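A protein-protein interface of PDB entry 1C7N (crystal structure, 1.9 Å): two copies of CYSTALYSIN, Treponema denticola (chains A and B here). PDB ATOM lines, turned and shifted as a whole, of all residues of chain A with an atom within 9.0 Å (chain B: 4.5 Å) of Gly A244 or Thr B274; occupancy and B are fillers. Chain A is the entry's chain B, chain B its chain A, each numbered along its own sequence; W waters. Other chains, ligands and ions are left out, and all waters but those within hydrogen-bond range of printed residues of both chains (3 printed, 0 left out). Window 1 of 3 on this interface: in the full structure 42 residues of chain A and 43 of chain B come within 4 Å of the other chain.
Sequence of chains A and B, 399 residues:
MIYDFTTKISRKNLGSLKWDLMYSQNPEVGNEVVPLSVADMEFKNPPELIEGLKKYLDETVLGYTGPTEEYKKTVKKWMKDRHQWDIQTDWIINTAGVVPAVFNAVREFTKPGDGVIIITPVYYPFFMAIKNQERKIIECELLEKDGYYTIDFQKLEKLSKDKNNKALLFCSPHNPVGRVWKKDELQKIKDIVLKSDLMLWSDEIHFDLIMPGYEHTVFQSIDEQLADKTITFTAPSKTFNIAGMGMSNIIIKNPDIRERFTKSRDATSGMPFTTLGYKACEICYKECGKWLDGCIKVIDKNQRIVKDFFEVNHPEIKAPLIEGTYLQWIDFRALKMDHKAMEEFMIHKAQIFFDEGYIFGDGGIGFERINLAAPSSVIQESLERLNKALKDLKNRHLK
O of Leu B62 lies within hydrogen-bond range of N of Ala A243, 3.3 Å away. The backbone carbonyl oxygen of Asn A241 lies close to the backbone carbonyl oxygen of Leu B62 (3.2 Å). The backbone NH of Thr B275 is in hydrogen-bond range of the backbone carbonyl oxygen of Gly A244 (3.2 Å). N of Gly A244 sits close to O of Gly B63 (3.4 Å). N of Leu B62 sits close to ND2 of Asn A45, 2.9 Å away. O of Leu B62 sits at hydrogen-bond distance from N of Gly A244, at 2.8 Å.
The backbone NH (N) of Ile A242 sits at hydrogen-bond distance from the backbone carbonyl oxygen (O) of Ser A237 (2.8 Å). The side-chain amide oxygen (OD1) of Asn A45 sits close to the backbone carbonyl oxygen (O) of Phe A240, 3.0 Å away. N of Gly B277 sits at hydrogen-bond distance from OG1 of Thr B274 (3.2 Å). OD1 of Asn A45 lies close to O of Asn A241 (2.9 Å). The guanidinium group of Arg A11 lies within salt-bridge range of the side-chain carboxylate of Asp A40 (3.0 Å).
Arg A11 touches Gly B63. CA of Gly B63 touches OD1 of Asp A40, 3.7 Å away. Leu B62 touches Ile A242 (O to CA, 3.3 Å). Ala A243 touches Phe B273 (O to CB, 3.9 Å). O of Phe B273 touches CA of Gly A244 (3.2 Å). O of Gly A244 touches CA of Thr B274, at 3.2 Å. SD of Met A245 touches CD1 of Leu B276, 3.8 Å away. CD1 of Leu B276 touches CD1 of Leu A276 (3.3 Å).
Of chain B, only Leu B62 (2.8 Å), Gly B63 (3.2 Å), Phe B273 (3.2 Å), Thr B274 (3.2 Å) and Thr B275 (3.2 Å) come within 4 Å of Gly A244. Thr B274 touches one residue of chain A. Of chain A, only Gly A244 comes within 4 Å of Thr B275. Printed residues of chain A within 4 Å of Leu B276: Met A245 (3.8 Å) and Leu A276 (3.3 Å). Of the printed residues of chain B, Arg A11 touches Gly B63 (3.99 Å). Printed residues of chain A within 4 Å of Phe B273: Ala A243 and Gly A244. Of the printed residues of chain B, Met A245 touches Leu B276 (3.8 Å). Thr A275 touches none of the printed residues of chain B. Tyr B278 touches none of the printed residues of chain A. The nearest residue of chain A that does not touch Thr B274 is Met A245 (5.0 Å).
Along chain A the printed residues that touch a printed residue of chain B span positions 11 to 276. Of the 12 printed residues of chain B, 6 touch a printed residue of chain A. Printed residues of chain B that touch a printed residue of chain A: Leu B62, Gly B63, Phe B273, Thr B274, Thr B275 and Leu B276. Among the printed residues, no Asp or Glu carboxylate lies within 4 Å of a Lys or Arg side-chain nitrogen of the other chain.
Met A245 touches Leu B276, but with the chains exchanged Leu A276 does not touch Met B245 (4.3 Å). Leu B276 touches its own counterpart, Leu A276. 7 positions are printed for both chains.
Water W2 lies within hydrogen-bond range of O of Gly A244 (2.7 Å), OG1 of Thr B274 (2.9 Å), N of Leu B276 (3.0 Å) and SD of Met A245 (3.5 Å). Water W3 lies within hydrogen-bond range of the side-chain hydroxyl (OG1) of Thr A274 (2.9 Å), the backbone NH (N) of Leu A276 (3.0 Å), the backbone NH (N) of Thr A275 (3.4 Å) and the side-chain sulfur (SD) of Met B245 (3.6 Å). Water W1 lies within hydrogen-bond range of OG1 of Thr B274 and OG1 of Thr A274.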
ATOM      1  N   ARG A  11     -20.306 -15.852  19.850  1.00  0.00           N
ATOM      2  CA  ARG A  11     -19.695 -14.534  19.969  1.00  0.00           C
ATOM      3  C   ARG A  11     -19.950 -13.952  21.354  1.00  0.00           C
ATOM      4  O   ARG A  11     -20.069 -12.740  21.521  1.00  0.00           O
ATOM      5  CB  ARG A  11     -20.236 -13.613  18.870  1.00  0.00           C
ATOM      6  CG  ARG A  11     -19.899 -14.107  17.473  1.00  0.00           C
ATOM      7  CD  ARG A  11     -20.681 -13.358  16.405  1.00  0.00           C
ATOM      8  NE  ARG A  11     -20.280 -11.957  16.278  1.00  0.00           N
ATOM      9  CZ  ARG A  11     -20.949 -11.061  15.557  1.00  0.00           C
ATOM     10  NH1 ARG A  11     -22.051 -11.420  14.904  1.00  0.00           N
ATOM     11  NH2 ARG A  11     -20.520  -9.807  15.487  1.00  0.00           N
ATOM     12  N   GLY A  15     -17.543  -8.619  22.493  1.00  0.00           N
ATOM     13  CA  GLY A  15     -17.824  -7.252  22.095  1.00  0.00           C
ATOM     14  C   GLY A  15     -18.858  -7.133  20.991  1.00  0.00           C
ATOM     15  O   GLY A  15     -19.037  -6.063  20.407  1.00  0.00           O
ATOM     16  N   LEU A  17     -22.201  -6.422  19.510  1.00  0.00           N
ATOM     17  CA  LEU A  17     -23.361  -5.639  19.930  1.00  0.00           C
ATOM     18  C   LEU A  17     -24.616  -6.501  19.982  1.00  0.00           C
ATOM     19  O   LEU A  17     -25.412  -6.407  20.916  1.00  0.00           O
ATOM     20  CB  LEU A  17     -23.597  -4.467  18.971  1.00  0.00           C
ATOM     21  CG  LEU A  17     -22.833  -3.166  19.244  1.00  0.00           C
ATOM     22  CD1 LEU A  17     -23.445  -2.453  20.441  1.00  0.00           C
ATOM     23  CD2 LEU A  17     -21.369  -3.473  19.489  1.00  0.00           C
ATOM     24  N   ALA A  39     -28.221  -6.766  12.167  1.00  0.00           N
ATOM     25  CA  ALA A  39     -27.787  -7.171  10.837  1.00  0.00           C
ATOM     26  C   ALA A  39     -26.297  -7.308  10.534  1.00  0.00           C
ATOM     27  O   ALA A  39     -25.709  -6.470   9.850  1.00  0.00           O
ATOM     28  CB  ALA A  39     -28.443  -6.267   9.782  1.00  0.00           C
ATOM     29  N   ASP A  40     -25.685  -8.355  11.074  1.00  0.00           N
ATOM     30  CA  ASP A  40     -24.306  -8.698  10.755  1.00  0.00           C
ATOM     31  C   ASP A  40     -24.398 -10.219  10.741  1.00  0.00           C
ATOM     32  O   ASP A  40     -25.290 -10.787  11.378  1.00  0.00           O
ATOM     33  CB  ASP A  40     -23.271  -8.098  11.742  1.00  0.00           C
ATOM     34  CG  ASP A  40     -23.278  -8.727  13.121  1.00  0.00           C
ATOM     35  OD1 ASP A  40     -22.583  -8.151  13.995  1.00  0.00           O
ATOM     36  OD2 ASP A  40     -23.940  -9.765  13.341  1.00  0.00           O
ATOM     37  N   ASN A  45     -15.767 -14.355   8.168  1.00  0.00           N
ATOM     38  CA  ASN A  45     -15.521 -13.568   6.967  1.00  0.00           C
ATOM     39  C   ASN A  45     -14.864 -14.358   5.841  1.00  0.00           C
ATOM     40  O   ASN A  45     -14.328 -15.447   6.064  1.00  0.00           O
ATOM     41  CB  ASN A  45     -14.674 -12.350   7.332  1.00  0.00           C
ATOM     42  CG  ASN A  45     -15.461 -11.324   8.131  1.00  0.00           C
ATOM     43  OD1 ASN A  45     -16.220 -10.522   7.570  1.00  0.00           O
ATOM     44  ND2 ASN A  45     -15.302 -11.359   9.449  1.00  0.00           N
ATOM     45  N   LEU A  53      -5.831  -9.422   4.598  1.00  0.00           N
ATOM     46  CA  LEU A  53      -5.573  -8.458   5.660  1.00  0.00           C
ATOM     47  C   LEU A  53      -4.335  -8.838   6.465  1.00  0.00           C
ATOM     48  O   LEU A  53      -3.562  -7.967   6.865  1.00  0.00           O
ATOM     49  CB  LEU A  53      -6.788  -8.344   6.580  1.00  0.00           C
ATOM     50  CG  LEU A  53      -8.027  -7.713   5.944  1.00  0.00           C
ATOM     51  CD1 LEU A  53      -9.211  -7.843   6.891  1.00  0.00           C
ATOM     52  CD2 LEU A  53      -7.741  -6.246   5.612  1.00  0.00           C
ATOM     53  N   ALA A  96     -17.151   6.858   7.747  1.00  0.00           N
ATOM     54  CA  ALA A  96     -16.997   5.663   8.566  1.00  0.00           C
ATOM     55  C   ALA A  96     -18.368   5.090   8.880  1.00  0.00           C
ATOM     56  O   ALA A  96     -18.804   5.089  10.033  1.00  0.00           O
ATOM     57  CB  ALA A  96     -16.257   5.993   9.860  1.00  0.00           C
ATOM     58  N   GLY A  97     -19.040   4.609   7.843  1.00  0.00           N
ATOM     59  CA  GLY A  97     -20.366   4.040   8.006  1.00  0.00           C
ATOM     60  C   GLY A  97     -21.414   4.836   7.248  1.00  0.00           C
ATOM     61  O   GLY A  97     -21.266   6.044   7.036  1.00  0.00           O
ATOM     62  N   PRO A 236     -19.187  -1.913   1.522  1.00  0.00           N
ATOM     63  CA  PRO A 236     -19.024  -3.363   1.381  1.00  0.00           C
ATOM     64  C   PRO A 236     -19.375  -4.107   2.664  1.00  0.00           C
ATOM     65  O   PRO A 236     -19.361  -5.332   2.693  1.00  0.00           O
ATOM     66  CB  PRO A 236     -17.539  -3.500   1.059  1.00  0.00           C
ATOM     67  CG  PRO A 236     -16.942  -2.439   1.956  1.00  0.00           C
ATOM     68  CD  PRO A 236     -17.880  -1.259   1.732  1.00  0.00           C
ATOM     69  N   SER A 237     -19.701  -3.356   3.713  1.00  0.00           N
ATOM     70  CA  SER A 237     -19.997  -3.923   5.030  1.00  0.00           C
ATOM     71  C   SER A 237     -21.105  -4.968   5.142  1.00  0.00           C
ATOM     72  O   SER A 237     -20.889  -6.040   5.711  1.00  0.00           O
ATOM     73  CB  SER A 237     -20.254  -2.787   6.029  1.00  0.00           C
ATOM     74  OG  SER A 237     -21.326  -1.960   5.613  1.00  0.00           O
ATOM     75  N   LYS A 238     -22.289  -4.672   4.626  1.00  0.00           N
ATOM     76  CA  LYS A 238     -23.383  -5.638   4.707  1.00  0.00           C
ATOM     77  C   LYS A 238     -23.075  -6.837   3.821  1.00  0.00           C
ATOM     78  O   LYS A 238     -23.276  -7.987   4.219  1.00  0.00           O
ATOM     79  CB  LYS A 238     -24.701  -4.985   4.279  1.00  0.00           C
ATOM     80  CG  LYS A 238     -25.845  -5.153   5.273  1.00  0.00           C
ATOM     81  CD  LYS A 238     -25.376  -4.947   6.708  1.00  0.00           C
ATOM     82  CE  LYS A 238     -26.519  -4.555   7.617  1.00  0.00           C
ATOM     83  NZ  LYS A 238     -26.968  -3.226   7.201  1.00  0.00           N
ATOM     84  N   PHE A 240     -20.105  -8.196   2.721  1.00  0.00           N
ATOM     85  CA  PHE A 240     -19.090  -9.128   3.194  1.00  0.00           C
ATOM     86  C   PHE A 240     -18.965  -9.249   4.712  1.00  0.00           C
ATOM     87  O   PHE A 240     -17.958  -9.742   5.219  1.00  0.00           O
ATOM     88  CB  PHE A 240     -17.732  -8.762   2.593  1.00  0.00           C
ATOM     89  CG  PHE A 240     -17.735  -8.692   1.089  1.00  0.00           C
ATOM     90  CD1 PHE A 240     -17.840  -7.465   0.437  1.00  0.00           C
ATOM     91  CD2 PHE A 240     -17.660  -9.854   0.325  1.00  0.00           C
ATOM     92  CE1 PHE A 240     -17.873  -7.398  -0.959  1.00  0.00           C
ATOM     93  CE2 PHE A 240     -17.693  -9.797  -1.067  1.00  0.00           C
ATOM     94  CZ  PHE A 240     -17.800  -8.564  -1.710  1.00  0.00           C
ATOM     95  N   ASN A 241     -19.987  -8.796   5.429  1.00  0.00           N
ATOM     96  CA  ASN A 241     -20.015  -8.865   6.884  1.00  0.00           C
ATOM     97  C   ASN A 241     -18.862  -8.121   7.551  1.00  0.00           C
ATOM     98  O   ASN A 241     -18.224  -8.643   8.472  1.00  0.00           O
ATOM     99  CB  ASN A 241     -20.015 -10.333   7.331  1.00  0.00           C
ATOM    100  CG  ASN A 241     -20.360 -10.501   8.796  1.00  0.00           C
ATOM    101  OD1 ASN A 241     -21.036  -9.660   9.390  1.00  0.00           O
ATOM    102  ND2 ASN A 241     -19.923 -11.608   9.380  1.00  0.00           N
ATOM    103  N   ILE A 242     -18.589  -6.902   7.096  1.00  0.00           N
ATOM    104  CA  ILE A 242     -17.507  -6.136   7.693  1.00  0.00           C
ATOM    105  C   ILE A 242     -17.925  -4.780   8.225  1.00  0.00           C
ATOM    106  O   ILE A 242     -17.243  -3.776   8.004  1.00  0.00           O
ATOM    107  CB  ILE A 242     -16.300  -5.954   6.723  1.00  0.00           C
ATOM    108  CG1 ILE A 242     -16.735  -5.284   5.421  1.00  0.00           C
ATOM    109  CG2 ILE A 242     -15.654  -7.303   6.443  1.00  0.00           C
ATOM    110  CD1 ILE A 242     -15.571  -5.090   4.429  1.00  0.00           C
ATOM    111  N   ALA A 243     -19.047  -4.756   8.942  1.00  0.00           N
ATOM    112  CA  ALA A 243     -19.544  -3.534   9.553  1.00  0.00           C
ATOM    113  C   ALA A 243     -18.523  -3.076  10.589  1.00  0.00           C
ATOM    114  O   ALA A 243     -18.576  -1.944  11.071  1.00  0.00           O
ATOM    115  CB  ALA A 243     -20.879  -3.791  10.232  1.00  0.00           C
ATOM    116  N   GLY A 244     -17.605  -3.976  10.933  1.00  0.00           N
ATOM    117  CA  GLY A 244     -16.583  -3.662  11.916  1.00  0.00           C
ATOM    118  C   GLY A 244     -15.292  -3.127  11.321  1.00  0.00           C
ATOM    119  O   GLY A 244     -14.289  -2.992  12.029  1.00  0.00           O
ATOM    120  N   MET A 245     -15.306  -2.827  10.026  1.00  0.00           N
ATOM    121  CA  MET A 245     -14.125  -2.289   9.357  1.00  0.00           C
ATOM    122  C   MET A 245     -14.263  -0.793   9.057  1.00  0.00           C
ATOM    123  O   MET A 245     -13.315  -0.150   8.591  1.00  0.00           O
ATOM    124  CB  MET A 245     -13.848  -3.067   8.074  1.00  0.00           C
ATOM    125  CG  MET A 245     -13.370  -4.486   8.344  1.00  0.00           C
ATOM    126  SD  MET A 245     -11.878  -4.501   9.364  1.00  0.00           S
ATOM    127  CE  MET A 245     -10.630  -4.673   8.112  1.00  0.00           C
ATOM    128  N   GLY A 246     -15.450  -0.260   9.336  1.00  0.00           N
ATOM    129  CA  GLY A 246     -15.739   1.155   9.141  1.00  0.00           C
ATOM    130  C   GLY A 246     -15.282   1.863   7.876  1.00  0.00           C
ATOM    131  O   GLY A 246     -14.422   2.750   7.936  1.00  0.00           O
ATOM    132  N   MET A 247     -15.859   1.499   6.734  1.00  0.00           N
ATOM    133  CA  MET A 247     -15.498   2.150   5.475  1.00  0.00           C
ATOM    134  C   MET A 247     -16.678   2.156   4.516  1.00  0.00           C
ATOM    135  O   MET A 247     -17.176   1.101   4.128  1.00  0.00           O
ATOM    136  CB  MET A 247     -14.299   1.448   4.829  1.00  0.00           C
ATOM    137  CG  MET A 247     -13.782   2.112   3.553  1.00  0.00           C
ATOM    138  SD  MET A 247     -13.507   3.906   3.672  1.00  0.00           S
ATOM    139  CE  MET A 247     -12.406   4.038   5.059  1.00  0.00           C
ATOM    140  N   THR A 274      -8.556   5.163   8.712  1.00  0.00           N
ATOM    141  CA  THR A 274      -8.444   3.718   8.883  1.00  0.00           C
ATOM    142  C   THR A 274      -7.709   3.020   7.742  1.00  0.00           C
ATOM    143  O   THR A 274      -8.225   2.905   6.633  1.00  0.00           O
ATOM    144  CB  THR A 274      -9.835   3.076   9.039  1.00  0.00           C
ATOM    145  OG1 THR A 274      -9.717   1.650   8.949  1.00  0.00           O
ATOM    146  CG2 THR A 274     -10.781   3.580   7.963  1.00  0.00           C
ATOM    147  N   THR A 275      -6.508   2.537   8.032  1.00  0.00           N
ATOM    148  CA  THR A 275      -5.693   1.852   7.040  1.00  0.00           C
ATOM    149  C   THR A 275      -6.362   0.571   6.532  1.00  0.00           C
ATOM    150  O   THR A 275      -6.476   0.362   5.322  1.00  0.00           O
ATOM    151  CB  THR A 275      -4.321   1.471   7.620  1.00  0.00           C
ATOM    152  OG1 THR A 275      -4.476   0.367   8.521  1.00  0.00           O
ATOM    153  CG2 THR A 275      -3.721   2.639   8.388  1.00  0.00           C
ATOM    154  N   LEU A 276      -6.814  -0.277   7.453  1.00  0.00           N
ATOM    155  CA  LEU A 276      -7.442  -1.542   7.072  1.00  0.00           C
ATOM    156  C   LEU A 276      -8.833  -1.402   6.456  1.00  0.00           C
ATOM    157  O   LEU A 276      -9.303  -2.304   5.765  1.00  0.00           O
ATOM    158  CB  LEU A 276      -7.497  -2.484   8.279  1.00  0.00           C
ATOM    159  CG  LEU A 276      -6.140  -2.743   8.945  1.00  0.00           C
ATOM    160  CD1 LEU A 276      -6.305  -3.731  10.090  1.00  0.00           C
ATOM    161  CD2 LEU A 276      -5.154  -3.285   7.925  1.00  0.00           C
ATOM    162  N   GLY A 277      -9.487  -0.273   6.705  1.00  0.00           N
ATOM    163  CA  GLY A 277     -10.805  -0.052   6.138  1.00  0.00           C
ATOM    164  C   GLY A 277     -10.741   0.009   4.620  1.00  0.00           C
ATOM    165  O   GLY A 277     -11.545  -0.624   3.928  1.00  0.00           O
ATOM    166  N   ALA A 280      -9.587  -3.524   3.152  1.00  0.00           N
ATOM    167  CA  ALA A 280     -10.613  -4.557   3.246  1.00  0.00           C
ATOM    168  C   ALA A 280     -11.642  -4.460   2.123  1.00  0.00           C
ATOM    169  O   ALA A 280     -12.104  -5.483   1.597  1.00  0.00           O
ATOM    170  CB  ALA A 280     -11.303  -4.473   4.589  1.00  0.00           C
ATOM    171  N   LEU B  62     -15.810  -9.834  11.828  1.00  0.00           N
ATOM    172  CA  LEU B  62     -15.705  -8.382  11.734  1.00  0.00           C
ATOM    173  C   LEU B  62     -17.040  -7.629  11.686  1.00  0.00           C
ATOM    174  O   LEU B  62     -17.215  -6.715  10.880  1.00  0.00           O
ATOM    175  CB  LEU B  62     -14.844  -8.024  10.519  1.00  0.00           C
ATOM    176  CG  LEU B  62     -13.467  -8.705  10.458  1.00  0.00           C
ATOM    177  CD1 LEU B  62     -12.831  -8.454   9.106  1.00  0.00           C
ATOM    178  CD2 LEU B  62     -12.563  -8.193  11.585  1.00  0.00           C
ATOM    179  N   GLY B  63     -17.967  -7.998  12.567  1.00  0.00           N
ATOM    180  CA  GLY B  63     -19.274  -7.356  12.593  1.00  0.00           C
ATOM    181  C   GLY B  63     -19.375  -6.130  13.486  1.00  0.00           C
ATOM    182  O   GLY B  63     -18.364  -5.510  13.819  1.00  0.00           O
ATOM    183  N   MET B 245      -5.677   3.163  13.079  1.00  0.00           N
ATOM    184  CA  MET B 245      -6.506   2.163  13.737  1.00  0.00           C
ATOM    185  C   MET B 245      -7.720   2.831  14.379  1.00  0.00           C
ATOM    186  O   MET B 245      -8.581   2.165  14.958  1.00  0.00           O
ATOM    187  CB  MET B 245      -5.685   1.414  14.785  1.00  0.00           C
ATOM    188  CG  MET B 245      -4.620   0.519  14.161  1.00  0.00           C
ATOM    189  SD  MET B 245      -5.349  -0.654  12.999  1.00  0.00           S
ATOM    190  CE  MET B 245      -5.423  -2.145  13.987  1.00  0.00           C
ATOM    191  N   GLY B 246      -7.769   4.156  14.254  1.00  0.00           N
ATOM    192  CA  GLY B 246      -8.866   4.961  14.767  1.00  0.00           C
ATOM    193  C   GLY B 246      -9.621   4.516  16.007  1.00  0.00           C
ATOM    194  O   GLY B 246     -10.728   3.991  15.902  1.00  0.00           O
ATOM    195  N   MET B 247      -9.030   4.727  17.180  1.00  0.00           N
ATOM    196  CA  MET B 247      -9.684   4.371  18.437  1.00  0.00           C
ATOM    197  C   MET B 247      -9.144   5.236  19.566  1.00  0.00           C
ATOM    198  O   MET B 247      -7.947   5.222  19.850  1.00  0.00           O
ATOM    199  CB  MET B 247      -9.482   2.891  18.764  1.00  0.00           C
ATOM    200  CG  MET B 247     -10.210   2.431  20.029  1.00  0.00           C
ATOM    201  SD  MET B 247     -11.965   2.909  20.108  1.00  0.00           S
ATOM    202  CE  MET B 247     -12.665   1.930  18.773  1.00  0.00           C
ATOM    203  N   PRO B 272     -18.050   4.097  17.565  1.00  0.00           N
ATOM    204  CA  PRO B 272     -17.082   3.373  16.729  1.00  0.00           C
ATOM    205  C   PRO B 272     -17.372   1.873  16.784  1.00  0.00           C
ATOM    206  O   PRO B 272     -17.445   1.293  17.870  1.00  0.00           O
ATOM    207  CB  PRO B 272     -15.734   3.697  17.381  1.00  0.00           C
ATOM    208  CG  PRO B 272     -15.996   4.959  18.160  1.00  0.00           C
ATOM    209  CD  PRO B 272     -17.375   4.742  18.704  1.00  0.00           C
ATOM    210  N   PHE B 273     -17.538   1.246  15.624  1.00  0.00           N
ATOM    211  CA  PHE B 273     -17.812  -0.190  15.570  1.00  0.00           C
ATOM    212  C   PHE B 273     -16.590  -0.955  15.061  1.00  0.00           C
ATOM    213  O   PHE B 273     -16.674  -2.149  14.773  1.00  0.00           O
ATOM    214  CB  PHE B 273     -18.997  -0.475  14.634  1.00  0.00           C
ATOM    215  CG  PHE B 273     -20.272   0.220  15.025  1.00  0.00           C
ATOM    216  CD1 PHE B 273     -20.952   1.013  14.104  1.00  0.00           C
ATOM    217  CD2 PHE B 273     -20.796   0.081  16.306  1.00  0.00           C
ATOM    218  CE1 PHE B 273     -22.130   1.658  14.451  1.00  0.00           C
ATOM    219  CE2 PHE B 273     -21.978   0.721  16.665  1.00  0.00           C
ATOM    220  CZ  PHE B 273     -22.647   1.513  15.734  1.00  0.00           C
ATOM    221  N   THR B 274     -15.459  -0.265  14.961  1.00  0.00           N
ATOM    222  CA  THR B 274     -14.221  -0.853  14.459  1.00  0.00           C
ATOM    223  C   THR B 274     -13.577  -1.871  15.391  1.00  0.00           C
ATOM    224  O   THR B 274     -12.801  -1.512  16.281  1.00  0.00           O
ATOM    225  CB  THR B 274     -13.191   0.239  14.147  1.00  0.00           C
ATOM    226  OG1 THR B 274     -11.893  -0.352  14.022  1.00  0.00           O
ATOM    227  CG2 THR B 274     -13.178   1.285  15.243  1.00  0.00           C
ATOM    228  N   THR B 275     -13.886  -3.143  15.151  1.00  0.00           N
ATOM    229  CA  THR B 275     -13.384  -4.258  15.948  1.00  0.00           C
ATOM    230  C   THR B 275     -11.873  -4.311  16.148  1.00  0.00           C
ATOM    231  O   THR B 275     -11.399  -4.609  17.248  1.00  0.00           O
ATOM    232  CB  THR B 275     -13.820  -5.600  15.340  1.00  0.00           C
ATOM    233  OG1 THR B 275     -13.286  -6.674  16.122  1.00  0.00           O
ATOM    234  CG2 THR B 275     -13.319  -5.719  13.918  1.00  0.00           C
ATOM    235  N   LEU B 276     -11.114  -4.040  15.090  1.00  0.00           N
ATOM    236  CA  LEU B 276      -9.660  -4.078  15.197  1.00  0.00           C
ATOM    237  C   LEU B 276      -9.131  -2.913  16.023  1.00  0.00           C
ATOM    238  O   LEU B 276      -8.078  -3.022  16.651  1.00  0.00           O
ATOM    239  CB  LEU B 276      -9.026  -4.077  13.807  1.00  0.00           C
ATOM    240  CG  LEU B 276      -9.417  -5.305  12.978  1.00  0.00           C
ATOM    241  CD1 LEU B 276      -8.817  -5.208  11.585  1.00  0.00           C
ATOM    242  CD2 LEU B 276      -8.948  -6.568  13.691  1.00  0.00           C
ATOM    243  N   GLY B 277      -9.866  -1.804  16.020  1.00  0.00           N
ATOM    244  CA  GLY B 277      -9.455  -0.648  16.793  1.00  0.00           C
ATOM    245  C   GLY B 277      -9.476  -0.982  18.275  1.00  0.00           C
ATOM    246  O   GLY B 277      -8.544  -0.662  19.012  1.00  0.00           O
ATOM    247  N   TYR B 278     -10.543  -1.628  18.722  1.00  0.00           N
ATOM    248  CA  TYR B 278     -10.635  -2.005  20.123  1.00  0.00           C
ATOM    249  C   TYR B 278      -9.526  -2.980  20.503  1.00  0.00           C
ATOM    250  O   TYR B 278      -8.851  -2.787  21.510  1.00  0.00           O
ATOM    251  CB  TYR B 278     -11.999  -2.629  20.435  1.00  0.00           C
ATOM    252  CG  TYR B 278     -13.139  -1.642  20.362  1.00  0.00           C
ATOM    253  CD1 TYR B 278     -14.020  -1.642  19.282  1.00  0.00           C
ATOM    254  CD2 TYR B 278     -13.320  -0.682  21.356  1.00  0.00           C
ATOM    255  CE1 TYR B 278     -15.054  -0.711  19.194  1.00  0.00           C
ATOM    256  CE2 TYR B 278     -14.350   0.258  21.273  1.00  0.00           C
ATOM    257  CZ  TYR B 278     -15.211   0.235  20.192  1.00  0.00           C
ATOM    258  OH  TYR B 278     -16.237   1.149  20.109  1.00  0.00           O
HETATM  259  O   HOH W   1     -10.032  -0.689  11.371  1.00  0.00           O
HETATM  260  O   HOH W   2     -11.658  -2.797  12.419  1.00  0.00           O
HETATM  261  O   HOH W   3      -7.529   0.208  10.279  1.00  0.00           O
